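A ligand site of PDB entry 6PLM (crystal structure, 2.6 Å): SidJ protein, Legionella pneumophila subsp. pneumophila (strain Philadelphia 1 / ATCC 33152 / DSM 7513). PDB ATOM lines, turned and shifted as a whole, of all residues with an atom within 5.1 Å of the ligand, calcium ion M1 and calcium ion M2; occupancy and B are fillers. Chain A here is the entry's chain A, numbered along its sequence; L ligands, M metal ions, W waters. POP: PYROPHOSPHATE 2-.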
ATOM      1  N   ARG A 256       5.519 -16.694  -1.426  1.00  0.00           N
ATOM      2  CA  ARG A 256       5.877 -15.268  -1.215  1.00  0.00           C
ATOM      3  C   ARG A 256       5.846 -14.969   0.292  1.00  0.00           C
ATOM      4  O   ARG A 256       5.902 -13.782   0.648  1.00  0.00           O
ATOM      5  CB  ARG A 256       4.878 -14.379  -1.935  1.00  0.00           C
ATOM      6  CG  ARG A 256       3.422 -14.698  -1.605  1.00  0.00           C
ATOM      7  CD  ARG A 256       2.584 -13.450  -1.738  1.00  0.00           C
ATOM      8  NE  ARG A 256       1.199 -13.664  -1.373  1.00  0.00           N
ATOM      9  CZ  ARG A 256       0.177 -13.199  -2.076  1.00  0.00           C
ATOM     10  NH1 ARG A 256      -1.051 -13.441  -1.682  1.00  0.00           N
ATOM     11  NH2 ARG A 256       0.398 -12.492  -3.168  1.00  0.00           N
ATOM     12  N   THR A 257       5.727 -15.995   1.123  1.00  0.00           N
ATOM     13  CA  THR A 257       5.647 -15.807   2.600  1.00  0.00           C
ATOM     14  C   THR A 257       6.979 -16.210   3.233  1.00  0.00           C
ATOM     15  O   THR A 257       7.471 -17.321   2.919  1.00  0.00           O
ATOM     16  CB  THR A 257       4.495 -16.595   3.210  1.00  0.00           C
ATOM     17  OG1 THR A 257       3.309 -16.239   2.508  1.00  0.00           O
ATOM     18  CG2 THR A 257       4.314 -16.325   4.682  1.00  0.00           C
ATOM     19  N   LYS A 271       3.903 -12.291   4.771  1.00  0.00           N
ATOM     20  CA  LYS A 271       3.382 -12.577   3.459  1.00  0.00           C
ATOM     21  C   LYS A 271       3.577 -11.313   2.643  1.00  0.00           C
ATOM     22  O   LYS A 271       3.073 -10.274   3.050  1.00  0.00           O
ATOM     23  CB  LYS A 271       1.894 -12.916   3.575  1.00  0.00           C
ATOM     24  CG  LYS A 271       1.115 -13.027   2.284  1.00  0.00           C
ATOM     25  CD  LYS A 271      -0.265 -13.674   2.474  1.00  0.00           C
ATOM     26  CE  LYS A 271      -0.571 -14.638   1.367  1.00  0.00           C
ATOM     27  NZ  LYS A 271      -1.972 -15.112   1.432  1.00  0.00           N
ATOM     28  N   LYS A 274       2.638  -9.788  -4.154  1.00  0.00           N
ATOM     29  CA  LYS A 274       2.918 -10.266  -5.544  1.00  0.00           C
ATOM     30  C   LYS A 274       2.876  -9.082  -6.527  1.00  0.00           C
ATOM     31  O   LYS A 274       2.342  -8.005  -6.194  1.00  0.00           O
ATOM     32  CB  LYS A 274       1.835 -11.248  -5.999  1.00  0.00           C
ATOM     33  CG  LYS A 274       2.075 -12.741  -5.815  1.00  0.00           C
ATOM     34  CD  LYS A 274       0.759 -13.497  -5.861  1.00  0.00           C
ATOM     35  CE  LYS A 274       0.803 -14.849  -6.526  1.00  0.00           C
ATOM     36  NZ  LYS A 274       1.089 -15.938  -5.556  1.00  0.00           N
ATOM     37  N   GLU A 285      -7.541 -10.470   3.916  1.00  0.00           N
ATOM     38  CA  GLU A 285      -7.053 -11.690   4.620  1.00  0.00           C
ATOM     39  C   GLU A 285      -6.935 -11.303   6.114  1.00  0.00           C
ATOM     40  O   GLU A 285      -7.433 -12.031   7.014  1.00  0.00           O
ATOM     41  CB  GLU A 285      -5.814 -12.248   3.931  1.00  0.00           C
ATOM     42  CG  GLU A 285      -5.199 -13.437   4.651  1.00  0.00           C
ATOM     43  CD  GLU A 285      -4.037 -14.170   3.957  1.00  0.00           C
ATOM     44  OE1 GLU A 285      -3.743 -15.363   4.323  1.00  0.00           O
ATOM     45  OE2 GLU A 285      -3.435 -13.539   3.036  1.00  0.00           O
ATOM     46  N   TYR A 347       1.279 -12.337  10.355  1.00  0.00           N
ATOM     47  CA  TYR A 347       0.394 -13.098  11.233  1.00  0.00           C
ATOM     48  C   TYR A 347       1.193 -14.188  11.944  1.00  0.00           C
ATOM     49  O   TYR A 347       2.340 -14.443  11.602  1.00  0.00           O
ATOM     50  CB  TYR A 347      -0.792 -13.640  10.419  1.00  0.00           C
ATOM     51  CG  TYR A 347      -0.442 -14.648   9.370  1.00  0.00           C
ATOM     52  CD1 TYR A 347      -0.151 -14.279   8.067  1.00  0.00           C
ATOM     53  CD2 TYR A 347      -0.435 -15.992   9.685  1.00  0.00           C
ATOM     54  CE1 TYR A 347       0.181 -15.227   7.109  1.00  0.00           C
ATOM     55  CE2 TYR A 347      -0.104 -16.956   8.732  1.00  0.00           C
ATOM     56  CZ  TYR A 347       0.217 -16.565   7.445  1.00  0.00           C
ATOM     57  OH  TYR A 347       0.598 -17.527   6.564  1.00  0.00           O
ATOM     58  N   TYR A 356       0.572 -28.733   4.004  1.00  0.00           N
ATOM     59  CA  TYR A 356      -0.486 -28.965   3.036  1.00  0.00           C
ATOM     60  C   TYR A 356      -1.098 -30.325   3.372  1.00  0.00           C
ATOM     61  O   TYR A 356      -0.393 -31.262   3.776  1.00  0.00           O
ATOM     62  CB  TYR A 356       0.030 -28.803   1.592  1.00  0.00           C
ATOM     63  CG  TYR A 356       0.599 -27.431   1.269  1.00  0.00           C
ATOM     64  CD1 TYR A 356      -0.248 -26.361   0.997  1.00  0.00           C
ATOM     65  CD2 TYR A 356       1.968 -27.187   1.238  1.00  0.00           C
ATOM     66  CE1 TYR A 356       0.250 -25.090   0.728  1.00  0.00           C
ATOM     67  CE2 TYR A 356       2.484 -25.925   0.983  1.00  0.00           C
ATOM     68  CZ  TYR A 356       1.613 -24.869   0.720  1.00  0.00           C
ATOM     69  OH  TYR A 356       2.094 -23.601   0.478  1.00  0.00           O
ATOM     70  N   TYR A 436      -0.626 -26.727  -3.858  1.00  0.00           N
ATOM     71  CA  TYR A 436      -0.629 -25.597  -2.934  1.00  0.00           C
ATOM     72  C   TYR A 436      -2.025 -25.321  -2.388  1.00  0.00           C
ATOM     73  O   TYR A 436      -2.405 -24.155  -2.153  1.00  0.00           O
ATOM     74  CB  TYR A 436      -0.050 -24.360  -3.618  1.00  0.00           C
ATOM     75  CG  TYR A 436       1.365 -24.563  -4.123  1.00  0.00           C
ATOM     76  CD1 TYR A 436       2.345 -25.104  -3.305  1.00  0.00           C
ATOM     77  CD2 TYR A 436       1.714 -24.217  -5.416  1.00  0.00           C
ATOM     78  CE1 TYR A 436       3.640 -25.277  -3.749  1.00  0.00           C
ATOM     79  CE2 TYR A 436       3.002 -24.367  -5.866  1.00  0.00           C
ATOM     80  CZ  TYR A 436       3.964 -24.899  -5.039  1.00  0.00           C
ATOM     81  OH  TYR A 436       5.216 -25.095  -5.527  1.00  0.00           O
ATOM     82  N   ASN A 438      -5.280 -24.651  -0.291  1.00  0.00           N
ATOM     83  CA  ASN A 438      -5.415 -23.860   0.940  1.00  0.00           C
ATOM     84  C   ASN A 438      -6.095 -24.672   2.063  1.00  0.00           C
ATOM     85  O   ASN A 438      -6.690 -24.117   2.973  1.00  0.00           O
ATOM     86  CB  ASN A 438      -6.272 -22.603   0.793  1.00  0.00           C
ATOM     87  CG  ASN A 438      -5.759 -21.675  -0.256  1.00  0.00           C
ATOM     88  OD1 ASN A 438      -4.575 -21.654  -0.473  1.00  0.00           O
ATOM     89  ND2 ASN A 438      -6.628 -20.856  -0.837  1.00  0.00           N
ATOM     90  N   ARG A 440      -5.073 -27.017   5.087  1.00  0.00           N
ATOM     91  CA  ARG A 440      -3.856 -27.320   5.750  1.00  0.00           C
ATOM     92  C   ARG A 440      -4.126 -28.325   6.871  1.00  0.00           C
ATOM     93  O   ARG A 440      -5.276 -28.633   7.201  1.00  0.00           O
ATOM     94  CB  ARG A 440      -3.193 -26.041   6.261  1.00  0.00           C
ATOM     95  CG  ARG A 440      -3.159 -24.909   5.240  1.00  0.00           C
ATOM     96  CD  ARG A 440      -2.304 -25.222   4.018  1.00  0.00           C
ATOM     97  NE  ARG A 440      -2.271 -24.103   3.070  1.00  0.00           N
ATOM     98  CZ  ARG A 440      -1.663 -22.955   3.300  1.00  0.00           C
ATOM     99  NH1 ARG A 440      -1.064 -22.755   4.465  1.00  0.00           N
ATOM    100  NH2 ARG A 440      -1.690 -21.986   2.405  1.00  0.00           N
ATOM    101  N   ASP A 446      -5.598 -19.058   3.794  1.00  0.00           N
ATOM    102  CA  ASP A 446      -5.786 -18.124   2.694  1.00  0.00           C
ATOM    103  C   ASP A 446      -7.240 -17.632   2.700  1.00  0.00           C
ATOM    104  O   ASP A 446      -7.900 -17.676   1.688  1.00  0.00           O
ATOM    105  CB  ASP A 446      -5.361 -18.769   1.371  1.00  0.00           C
ATOM    106  CG  ASP A 446      -4.672 -17.843   0.376  1.00  0.00           C
ATOM    107  OD1 ASP A 446      -4.557 -16.649   0.688  1.00  0.00           O
ATOM    108  OD2 ASP A 446      -4.231 -18.327  -0.690  1.00  0.00           O
ATOM    109  N   ASP A 449      -9.233 -14.836   0.215  1.00  0.00           N
ATOM    110  CA  ASP A 449      -9.689 -15.296  -1.080  1.00  0.00           C
ATOM    111  C   ASP A 449     -11.088 -15.889  -0.933  1.00  0.00           C
ATOM    112  O   ASP A 449     -11.287 -17.083  -1.083  1.00  0.00           O
ATOM    113  CB  ASP A 449      -8.668 -16.261  -1.664  1.00  0.00           C
ATOM    114  CG  ASP A 449      -7.310 -15.653  -2.071  1.00  0.00           C
ATOM    115  OD1 ASP A 449      -7.154 -14.368  -2.190  1.00  0.00           O
ATOM    116  OD2 ASP A 449      -6.389 -16.466  -2.273  1.00  0.00           O
HETATM  117  P1  POP L   1      -0.642 -18.763   1.218  1.00  0.00           P
HETATM  118  O1  POP L   1      -0.806 -17.595   2.126  1.00  0.00           O
HETATM  119  O2  POP L   1      -1.920 -19.476   0.803  1.00  0.00           O
HETATM  120  O3  POP L   1       0.362 -19.750   1.787  1.00  0.00           O
HETATM  121  O   POP L   1      -0.012 -17.810   0.017  1.00  0.00           O
HETATM  122  P2  POP L   1      -0.768 -17.339  -1.348  1.00  0.00           P
HETATM  123  O4  POP L   1       0.309 -16.641  -2.209  1.00  0.00           O
HETATM  124  O5  POP L   1      -2.001 -16.418  -1.153  1.00  0.00           O
HETATM  125  O6  POP L   1      -1.105 -18.751  -1.757  1.00  0.00           O
HETATM  126 CA    CA M   1      -4.087 -16.120  -2.056  1.00  0.00          CA
HETATM  127 CA    CA M   2      -2.708 -20.256  -1.152  1.00  0.00          CA
HETATM  128  O   HOH W   1       2.905 -17.858  -1.397  1.00  0.00           O
HETATM  129  O   HOH W   2       0.480 -20.395  -3.961  1.00  0.00           O
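O3 of the ligand is in salt-bridge range of NH2 of Arg 440 (3.1 Å). The side-chain amino group (NZ) of Lys 274 lies within salt-bridge range of an oxygen (O4) of the ligand, 3.5 Å away. NZ of Lys 271 is in salt-bridge range of O1 of the ligand. The guanidinium group (NE) of Arg 256 lies within salt-bridge range of an oxygen (O4) of the ligand (3.2 Å).
The nearest printed residue that does not touch calcium ion M1 is Arg 256 (4.1 Å).
Two residues have an atom within 4 Å of calcium ion M2: Asn 438 and Asp 446. The nearest printed residue that does not touch calcium ion M2 is Tyr 436 (4.04 Å).
NZ of Lys 271 lies within salt-bridge range of OE2 of Glu 285 (2.7 Å). The side-chain amino group (NZ) of Lys 271 sits close to the side-chain carboxylate (OD1) of Asp 446 (3.1 Å).
Water W1 bridges the backbone NH (N) of Arg 256 (2.9 Å) and an oxygen (O4) of the ligand (3.0 Å).
Within 4 Å of the ligand: Arg 256, Lys 271, Lys 274, Asn 438, Arg 440 and Asp 446.
O2 of the ligand is bound to calcium ion M2. Calcium ion M2 is bound by an oxygen (O6) of the ligand (2.3 Å). OD1 of Asn 438 is bound to calcium ion M2. The side-chain carboxylate (OD2) of Asp 446 is bound to calcium ion M2, 2.5 Å away.
O5 of the ligand is bound to calcium ion M1 (2.3 Å). Calcium ion M1 is bound by OD2 of Asp 449, at 2.3 Å. The side-chain carboxylate (OD2) of Asp 446 binds calcium ion M1 (2.6 Å). Calcium ion M1 is bound by OD1 of Asp 446, at 2.8 Å.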
